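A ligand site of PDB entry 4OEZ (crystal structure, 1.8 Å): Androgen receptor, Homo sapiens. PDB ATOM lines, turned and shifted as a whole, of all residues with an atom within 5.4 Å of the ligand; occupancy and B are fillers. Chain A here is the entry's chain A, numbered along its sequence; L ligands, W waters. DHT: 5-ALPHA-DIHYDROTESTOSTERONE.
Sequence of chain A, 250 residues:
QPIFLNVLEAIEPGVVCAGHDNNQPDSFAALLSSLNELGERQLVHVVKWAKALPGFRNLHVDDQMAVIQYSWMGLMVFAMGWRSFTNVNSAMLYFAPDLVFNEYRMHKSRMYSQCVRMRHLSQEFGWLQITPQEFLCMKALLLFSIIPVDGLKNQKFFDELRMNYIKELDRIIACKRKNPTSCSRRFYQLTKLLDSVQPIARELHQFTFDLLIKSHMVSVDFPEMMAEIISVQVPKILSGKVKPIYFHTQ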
ATOM      1  N   LEU A  32     -33.074  -9.055  -2.833  1.00  0.00           N
ATOM      2  CA  LEU A  32     -32.979 -10.377  -3.473  1.00  0.00           C
ATOM      3  C   LEU A  32     -33.617 -10.328  -4.863  1.00  0.00           C
ATOM      4  O   LEU A  32     -33.164 -11.018  -5.757  1.00  0.00           O
ATOM      5  CB  LEU A  32     -33.567 -11.491  -2.579  1.00  0.00           C
ATOM      6  CG  LEU A  32     -32.548 -12.230  -1.711  1.00  0.00           C
ATOM      7  CD1 LEU A  32     -31.529 -13.108  -2.473  1.00  0.00           C
ATOM      8  CD2 LEU A  32     -31.759 -11.196  -0.891  1.00  0.00           C
ATOM      9  N   LEU A  35     -30.920  -9.008  -7.082  1.00  0.00           N
ATOM     10  CA  LEU A  35     -29.932 -10.102  -7.343  1.00  0.00           C
ATOM     11  C   LEU A  35     -30.435 -11.086  -8.359  1.00  0.00           C
ATOM     12  O   LEU A  35     -29.673 -11.531  -9.244  1.00  0.00           O
ATOM     13  CB  LEU A  35     -29.515 -10.823  -6.032  1.00  0.00           C
ATOM     14  CG  LEU A  35     -28.575 -10.000  -5.135  1.00  0.00           C
ATOM     15  CD1 LEU A  35     -28.300 -10.798  -3.820  1.00  0.00           C
ATOM     16  CD2 LEU A  35     -27.191  -9.781  -5.810  1.00  0.00           C
ATOM     17  N   ASN A  36     -31.723 -11.395  -8.294  1.00  0.00           N
ATOM     18  CA  ASN A  36     -32.324 -12.374  -9.234  1.00  0.00           C
ATOM     19  C   ASN A  36     -32.366 -11.801 -10.645  1.00  0.00           C
ATOM     20  O   ASN A  36     -32.037 -12.500 -11.610  1.00  0.00           O
ATOM     21  CB  ASN A  36     -33.724 -12.742  -8.793  1.00  0.00           C
ATOM     22  CG  ASN A  36     -33.749 -13.655  -7.601  1.00  0.00           C
ATOM     23  OD1 ASN A  36     -32.754 -14.393  -7.292  1.00  0.00           O
ATOM     24  ND2 ASN A  36     -34.915 -13.687  -6.927  1.00  0.00           N
ATOM     25  N   LEU A  38     -30.291  -9.478 -11.771  1.00  0.00           N
ATOM     26  CA  LEU A  38     -28.920  -9.438 -12.154  1.00  0.00           C
ATOM     27  C   LEU A  38     -28.508 -10.794 -12.699  1.00  0.00           C
ATOM     28  O   LEU A  38     -27.793 -10.900 -13.714  1.00  0.00           O
ATOM     29  CB  LEU A  38     -28.021  -9.055 -10.950  1.00  0.00           C
ATOM     30  CG  LEU A  38     -26.543  -8.838 -11.331  1.00  0.00           C
ATOM     31  CD1 LEU A  38     -26.327  -7.774 -12.443  1.00  0.00           C
ATOM     32  CD2 LEU A  38     -25.659  -8.507 -10.108  1.00  0.00           C
ATOM     33  N   GLY A  39     -28.936 -11.842 -11.985  1.00  0.00           N
ATOM     34  CA  GLY A  39     -28.549 -13.202 -12.423  1.00  0.00           C
ATOM     35  C   GLY A  39     -29.046 -13.428 -13.859  1.00  0.00           C
ATOM     36  O   GLY A  39     -28.362 -14.019 -14.678  1.00  0.00           O
ATOM     37  N   GLN A  42     -26.988 -11.352 -16.269  1.00  0.00           N
ATOM     38  CA  GLN A  42     -25.693 -11.972 -16.426  1.00  0.00           C
ATOM     39  C   GLN A  42     -25.766 -13.301 -17.188  1.00  0.00           C
ATOM     40  O   GLN A  42     -24.856 -13.620 -17.898  1.00  0.00           O
ATOM     41  CB  GLN A  42     -24.984 -12.203 -15.075  1.00  0.00           C
ATOM     42  CG  GLN A  42     -24.483 -10.864 -14.522  1.00  0.00           C
ATOM     43  CD  GLN A  42     -23.543 -10.925 -13.356  1.00  0.00           C
ATOM     44  OE1 GLN A  42     -23.242  -9.874 -12.721  1.00  0.00           O
ATOM     45  NE2 GLN A  42     -23.065 -12.142 -13.019  1.00  0.00           N
ATOM     46  N   TRP A  72     -23.201 -21.796 -13.851  1.00  0.00           N
ATOM     47  CA  TRP A  72     -23.359 -20.331 -13.843  1.00  0.00           C
ATOM     48  C   TRP A  72     -23.152 -19.706 -12.438  1.00  0.00           C
ATOM     49  O   TRP A  72     -22.608 -18.679 -12.327  1.00  0.00           O
ATOM     50  CB  TRP A  72     -24.748 -19.899 -14.416  1.00  0.00           C
ATOM     51  CG  TRP A  72     -25.930 -20.435 -13.638  1.00  0.00           C
ATOM     52  CD1 TRP A  72     -26.563 -21.654 -13.849  1.00  0.00           C
ATOM     53  CD2 TRP A  72     -26.579 -19.855 -12.492  1.00  0.00           C
ATOM     54  NE1 TRP A  72     -27.547 -21.861 -12.930  1.00  0.00           N
ATOM     55  CE2 TRP A  72     -27.613 -20.781 -12.092  1.00  0.00           C
ATOM     56  CE3 TRP A  72     -26.448 -18.657 -11.776  1.00  0.00           C
ATOM     57  CZ2 TRP A  72     -28.480 -20.525 -11.012  1.00  0.00           C
ATOM     58  CZ3 TRP A  72     -27.335 -18.396 -10.674  1.00  0.00           C
ATOM     59  CH2 TRP A  72     -28.349 -19.323 -10.319  1.00  0.00           C
ATOM     60  N   MET A  73     -23.546 -20.391 -11.368  1.00  0.00           N
ATOM     61  CA  MET A  73     -23.354 -19.805 -10.015  1.00  0.00           C
ATOM     62  C   MET A  73     -21.885 -19.606  -9.661  1.00  0.00           C
ATOM     63  O   MET A  73     -21.454 -18.482  -9.259  1.00  0.00           O
ATOM     64  CB  MET A  73     -24.009 -20.723  -8.961  1.00  0.00           C
ATOM     65  CG  MET A  73     -23.995 -20.079  -7.559  1.00  0.00           C
ATOM     66  SD  MET A  73     -25.201 -18.755  -7.313  1.00  0.00           S
ATOM     67  CE  MET A  73     -26.728 -19.661  -7.263  1.00  0.00           C
ATOM     68  N   MET A  76     -20.320 -16.826 -11.901  1.00  0.00           N
ATOM     69  CA  MET A  76     -20.775 -15.450 -11.609  1.00  0.00           C
ATOM     70  C   MET A  76     -20.241 -15.016 -10.252  1.00  0.00           C
ATOM     71  O   MET A  76     -19.954 -13.817 -10.030  1.00  0.00           O
ATOM     72  CB  MET A  76     -22.273 -15.444 -11.502  1.00  0.00           C
ATOM     73  CG  MET A  76     -22.966 -15.619 -12.902  1.00  0.00           C
ATOM     74  SD  MET A  76     -24.711 -15.402 -12.773  1.00  0.00           S
ATOM     75  CE  MET A  76     -25.243 -15.805 -14.460  1.00  0.00           C
ATOM     76  N   VAL A  77     -20.149 -15.991  -9.350  1.00  0.00           N
ATOM     77  CA  VAL A  77     -19.569 -15.704  -8.016  1.00  0.00           C
ATOM     78  C   VAL A  77     -18.072 -15.351  -8.198  1.00  0.00           C
ATOM     79  O   VAL A  77     -17.623 -14.334  -7.637  1.00  0.00           O
ATOM     80  CB  VAL A  77     -19.769 -16.880  -7.023  1.00  0.00           C
ATOM     81  CG1 VAL A  77     -18.832 -16.704  -5.811  1.00  0.00           C
ATOM     82  CG2 VAL A  77     -21.234 -17.040  -6.578  1.00  0.00           C
ATOM     83  N   MET A  80     -17.670 -12.030  -9.740  1.00  0.00           N
ATOM     84  CA  MET A  80     -18.091 -10.943  -8.861  1.00  0.00           C
ATOM     85  C   MET A  80     -16.966 -10.730  -7.851  1.00  0.00           C
ATOM     86  O   MET A  80     -16.606  -9.553  -7.471  1.00  0.00           O
ATOM     87  CB  MET A  80     -19.357 -11.371  -8.137  1.00  0.00           C
ATOM     88  CG  MET A  80     -19.910 -10.327  -7.141  1.00  0.00           C
ATOM     89  SD  MET A  80     -19.169 -10.261  -5.500  1.00  0.00           S
ATOM     90  CE  MET A  80     -19.915 -11.748  -4.800  1.00  0.00           C
ATOM     91  N   ARG A  83     -14.427  -8.608  -9.580  1.00  0.00           N
ATOM     92  CA  ARG A  83     -14.929  -7.201  -9.631  1.00  0.00           C
ATOM     93  C   ARG A  83     -14.727  -6.503  -8.295  1.00  0.00           C
ATOM     94  O   ARG A  83     -14.302  -5.298  -8.243  1.00  0.00           O
ATOM     95  CB  ARG A  83     -16.461  -7.149  -9.972  1.00  0.00           C
ATOM     96  CG  ARG A  83     -16.762  -7.331 -11.422  1.00  0.00           C
ATOM     97  CD  ARG A  83     -18.203  -6.966 -11.786  1.00  0.00           C
ATOM     98  NE  ARG A  83     -19.252  -7.724 -11.099  1.00  0.00           N
ATOM     99  CZ  ARG A  83     -19.621  -8.964 -11.424  1.00  0.00           C
ATOM    100  NH1 ARG A  83     -19.014  -9.669 -12.400  1.00  0.00           N
ATOM    101  NH2 ARG A  83     -20.630  -9.518 -10.720  1.00  0.00           N
ATOM    102  N   PHE A  95     -21.511  -6.586  -6.814  1.00  0.00           N
ATOM    103  CA  PHE A  95     -22.377  -7.392  -7.700  1.00  0.00           C
ATOM    104  C   PHE A  95     -22.539  -6.645  -9.038  1.00  0.00           C
ATOM    105  O   PHE A  95     -22.473  -7.247 -10.105  1.00  0.00           O
ATOM    106  CB  PHE A  95     -23.720  -7.670  -7.037  1.00  0.00           C
ATOM    107  CG  PHE A  95     -23.615  -8.576  -5.840  1.00  0.00           C
ATOM    108  CD1 PHE A  95     -23.701  -8.103  -4.555  1.00  0.00           C
ATOM    109  CD2 PHE A  95     -23.495  -9.937  -6.061  1.00  0.00           C
ATOM    110  CE1 PHE A  95     -23.610  -8.996  -3.451  1.00  0.00           C
ATOM    111  CE2 PHE A  95     -23.389 -10.830  -4.990  1.00  0.00           C
ATOM    112  CZ  PHE A  95     -23.422 -10.355  -3.676  1.00  0.00           C
ATOM    113  N   MET A 111     -28.175 -13.416   3.917  1.00  0.00           N
ATOM    114  CA  MET A 111     -27.140 -14.216   3.294  1.00  0.00           C
ATOM    115  C   MET A 111     -25.819 -13.858   3.860  1.00  0.00           C
ATOM    116  O   MET A 111     -24.767 -13.970   3.206  1.00  0.00           O
ATOM    117  CB  MET A 111     -27.067 -13.843   1.813  1.00  0.00           C
ATOM    118  CG  MET A 111     -28.120 -14.478   1.004  1.00  0.00           C
ATOM    119  SD  MET A 111     -27.589 -14.696  -0.714  1.00  0.00           S
ATOM    120  CE  MET A 111     -26.928 -13.072  -0.994  1.00  0.00           C
ATOM    121  N   MET A 118     -17.964 -15.034   0.262  1.00  0.00           N
ATOM    122  CA  MET A 118     -17.597 -14.406  -1.017  1.00  0.00           C
ATOM    123  C   MET A 118     -16.605 -13.271  -0.877  1.00  0.00           C
ATOM    124  O   MET A 118     -15.739 -13.076  -1.702  1.00  0.00           O
ATOM    125  CB  MET A 118     -18.878 -13.947  -1.760  1.00  0.00           C
ATOM    126  CG  MET A 118     -19.810 -15.086  -2.091  1.00  0.00           C
ATOM    127  SD  MET A 118     -21.135 -14.607  -3.212  1.00  0.00           S
ATOM    128  CE  MET A 118     -22.388 -13.987  -2.101  1.00  0.00           C
ATOM    129  N   LEU A 204     -25.086 -21.311  -2.000  1.00  0.00           N
ATOM    130  CA  LEU A 204     -25.944 -20.385  -2.707  1.00  0.00           C
ATOM    131  C   LEU A 204     -26.994 -21.131  -3.477  1.00  0.00           C
ATOM    132  O   LEU A 204     -28.101 -20.677  -3.600  1.00  0.00           O
ATOM    133  CB  LEU A 204     -25.051 -19.500  -3.636  1.00  0.00           C
ATOM    134  CG  LEU A 204     -24.313 -18.388  -2.906  1.00  0.00           C
ATOM    135  CD1 LEU A 204     -23.270 -17.684  -3.748  1.00  0.00           C
ATOM    136  CD2 LEU A 204     -25.168 -17.378  -2.133  1.00  0.00           C
ATOM    137  N   PHE A 207     -29.600 -21.926  -0.965  1.00  0.00           N
ATOM    138  CA  PHE A 207     -30.265 -20.665  -0.543  1.00  0.00           C
ATOM    139  C   PHE A 207     -31.274 -20.221  -1.568  1.00  0.00           C
ATOM    140  O   PHE A 207     -32.420 -19.898  -1.279  1.00  0.00           O
ATOM    141  CB  PHE A 207     -29.243 -19.541  -0.273  1.00  0.00           C
ATOM    142  CG  PHE A 207     -29.883 -18.319   0.337  1.00  0.00           C
ATOM    143  CD1 PHE A 207     -30.477 -17.333  -0.461  1.00  0.00           C
ATOM    144  CD2 PHE A 207     -29.923 -18.181   1.727  1.00  0.00           C
ATOM    145  CE1 PHE A 207     -31.071 -16.202   0.116  1.00  0.00           C
ATOM    146  CE2 PHE A 207     -30.563 -17.076   2.328  1.00  0.00           C
ATOM    147  CZ  PHE A 207     -31.148 -16.086   1.510  1.00  0.00           C
ATOM    148  N   THR A 208     -30.862 -20.213  -2.843  1.00  0.00           N
ATOM    149  CA  THR A 208     -31.741 -19.757  -3.888  1.00  0.00           C
ATOM    150  C   THR A 208     -32.914 -20.714  -4.119  1.00  0.00           C
ATOM    151  O   THR A 208     -34.056 -20.276  -4.423  1.00  0.00           O
ATOM    152  CB  THR A 208     -30.941 -19.416  -5.209  1.00  0.00           C
ATOM    153  OG1 THR A 208     -31.782 -18.687  -6.089  1.00  0.00           O
ATOM    154  CG2 THR A 208     -30.503 -20.689  -5.922  1.00  0.00           C
ATOM    155  N   LEU A 211     -35.360 -20.151  -1.326  1.00  0.00           N
ATOM    156  CA  LEU A 211     -35.965 -18.884  -1.609  1.00  0.00           C
ATOM    157  C   LEU A 211     -36.981 -19.006  -2.723  1.00  0.00           C
ATOM    158  O   LEU A 211     -38.049 -18.460  -2.631  1.00  0.00           O
ATOM    159  CB  LEU A 211     -34.883 -17.841  -1.988  1.00  0.00           C
ATOM    160  CG  LEU A 211     -35.353 -16.392  -2.127  1.00  0.00           C
ATOM    161  CD1 LEU A 211     -36.174 -15.934  -0.919  1.00  0.00           C
ATOM    162  CD2 LEU A 211     -34.128 -15.524  -2.377  1.00  0.00           C
ATOM    163  N   PHE A 222     -38.621 -13.828  -8.916  1.00  0.00           N
ATOM    164  CA  PHE A 222     -37.683 -14.549  -9.802  1.00  0.00           C
ATOM    165  C   PHE A 222     -38.085 -14.415 -11.236  1.00  0.00           C
ATOM    166  O   PHE A 222     -39.173 -14.838 -11.595  1.00  0.00           O
ATOM    167  CB  PHE A 222     -37.705 -16.066  -9.478  1.00  0.00           C
ATOM    168  CG  PHE A 222     -36.919 -16.443  -8.269  1.00  0.00           C
ATOM    169  CD1 PHE A 222     -37.445 -16.261  -6.959  1.00  0.00           C
ATOM    170  CD2 PHE A 222     -35.662 -16.969  -8.413  1.00  0.00           C
ATOM    171  CE1 PHE A 222     -36.680 -16.584  -5.815  1.00  0.00           C
ATOM    172  CE2 PHE A 222     -34.912 -17.314  -7.294  1.00  0.00           C
ATOM    173  CZ  PHE A 222     -35.403 -17.116  -5.982  1.00  0.00           C
ATOM    174  N   MET A 226     -34.454 -17.840 -14.597  1.00  0.00           N
ATOM    175  CA  MET A 226     -33.956 -18.168 -13.265  1.00  0.00           C
ATOM    176  C   MET A 226     -34.876 -19.162 -12.559  1.00  0.00           C
ATOM    177  O   MET A 226     -34.382 -20.118 -12.008  1.00  0.00           O
ATOM    178  CB  MET A 226     -33.828 -16.919 -12.373  1.00  0.00           C
ATOM    179  CG  MET A 226     -32.811 -15.882 -12.832  1.00  0.00           C
ATOM    180  SD  MET A 226     -31.274 -16.623 -13.411  1.00  0.00           S
ATOM    181  CE  MET A 226     -30.539 -16.642 -11.934  1.00  0.00           C
ATOM    182  N   ILE A 230     -33.598 -22.813 -11.640  1.00  0.00           N
ATOM    183  CA  ILE A 230     -33.440 -23.146 -10.228  1.00  0.00           C
ATOM    184  C   ILE A 230     -34.389 -24.292  -9.806  1.00  0.00           C
ATOM    185  O   ILE A 230     -34.104 -24.990  -8.847  1.00  0.00           O
ATOM    186  CB  ILE A 230     -33.629 -21.897  -9.363  1.00  0.00           C
ATOM    187  CG1 ILE A 230     -32.501 -20.921  -9.688  1.00  0.00           C
ATOM    188  CG2 ILE A 230     -33.766 -22.271  -7.862  1.00  0.00           C
ATOM    189  CD1 ILE A 230     -32.644 -19.560  -9.028  1.00  0.00           C
HETATM  190  C1  DHT L   1     -25.925 -12.684  -9.480  1.00  0.00           C
HETATM  191  C2  DHT L   1     -24.619 -12.336 -10.219  1.00  0.00           C
HETATM  192  C3  DHT L   1     -23.445 -12.105  -9.293  1.00  0.00           C
HETATM  193  O3  DHT L   1     -22.682 -11.134  -9.455  1.00  0.00           O
HETATM  194  C4  DHT L   1     -23.225 -13.066  -8.148  1.00  0.00           C
HETATM  195  C5  DHT L   1     -24.570 -13.362  -7.458  1.00  0.00           C
HETATM  196  C6  DHT L   1     -24.265 -14.352  -6.319  1.00  0.00           C
HETATM  197  C7  DHT L   1     -25.541 -14.611  -5.524  1.00  0.00           C
HETATM  198  C8  DHT L   1     -26.772 -14.953  -6.374  1.00  0.00           C
HETATM  199  C9  DHT L   1     -26.973 -13.934  -7.546  1.00  0.00           C
HETATM  200  C10 DHT L   1     -25.723 -13.810  -8.419  1.00  0.00           C
HETATM  201  C11 DHT L   1     -28.244 -14.313  -8.336  1.00  0.00           C
HETATM  202  C12 DHT L   1     -29.563 -14.474  -7.568  1.00  0.00           C
HETATM  203  C13 DHT L   1     -29.304 -15.377  -6.372  1.00  0.00           C
HETATM  204  C14 DHT L   1     -28.041 -14.923  -5.568  1.00  0.00           C
HETATM  205  C15 DHT L   1     -28.025 -15.814  -4.310  1.00  0.00           C
HETATM  206  C16 DHT L   1     -29.536 -15.925  -4.055  1.00  0.00           C
HETATM  207  C17 DHT L   1     -30.300 -15.294  -5.218  1.00  0.00           C
HETATM  208  O17 DHT L   1     -31.520 -16.007  -5.475  1.00  0.00           O
HETATM  209  C18 DHT L   1     -29.222 -16.860  -6.871  1.00  0.00           C
HETATM  210  C19 DHT L   1     -25.359 -15.079  -9.264  1.00  0.00           C
HETATM  211  O   HOH W   1     -20.613 -12.097 -11.960  1.00  0.00           O
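OD1 of Asn 36 lies within hydrogen-bond range of O17 of the ligand (2.7 Å).
O17 of the ligand sits at hydrogen-bond distance from OG1 of Thr 208, at 2.8 Å.
NH2 of Arg 83 is in hydrogen-bond range of O3 of the ligand (2.9 Å).
ND2 of Asn 36 lies close to O of Leu 32 (3.4 Å).
The side-chain amide oxygen of Gln 42 is in hydrogen-bond range of the guanidinium group of Arg 83 (3.3 Å).
O of Phe 95 sits at hydrogen-bond distance from NH2 of Arg 83 (3.0 Å).
NE2 of Gln 42 lies close to SD of Met 76.
Residues that only touch the ligand: Gln 42 (3.2 Å), Leu 35 (3.3 Å), Met 76 (3.6 Å), Met 80 (3.6 Å), Phe 95 (3.7 Å), Leu 32 (3.7 Å), Met 73 (3.8 Å), Met 111 (3.8 Å), Leu 204 (3.9 Å), Leu 38 (3.97 Å), Phe 207 (3.97 Å) and Gly 39 (3.98 Å).
15 residues have an atom within 4 Å of the ligand: Leu 32, Leu 35, Asn 36, Leu 38, Gly 39, Gln 42, Met 73, Met 76, Met 80, Arg 83, Phe 95, Met 111, Leu 204, Phe 207 and Thr 208.
The nearest printed residue that does not touch the ligand is Val 77 (4.1 Å).
Water W1 lies within hydrogen-bond range of O of Met 76, NE2 of Gln 42, NH2 of Arg 83 and O3 of the ligand.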
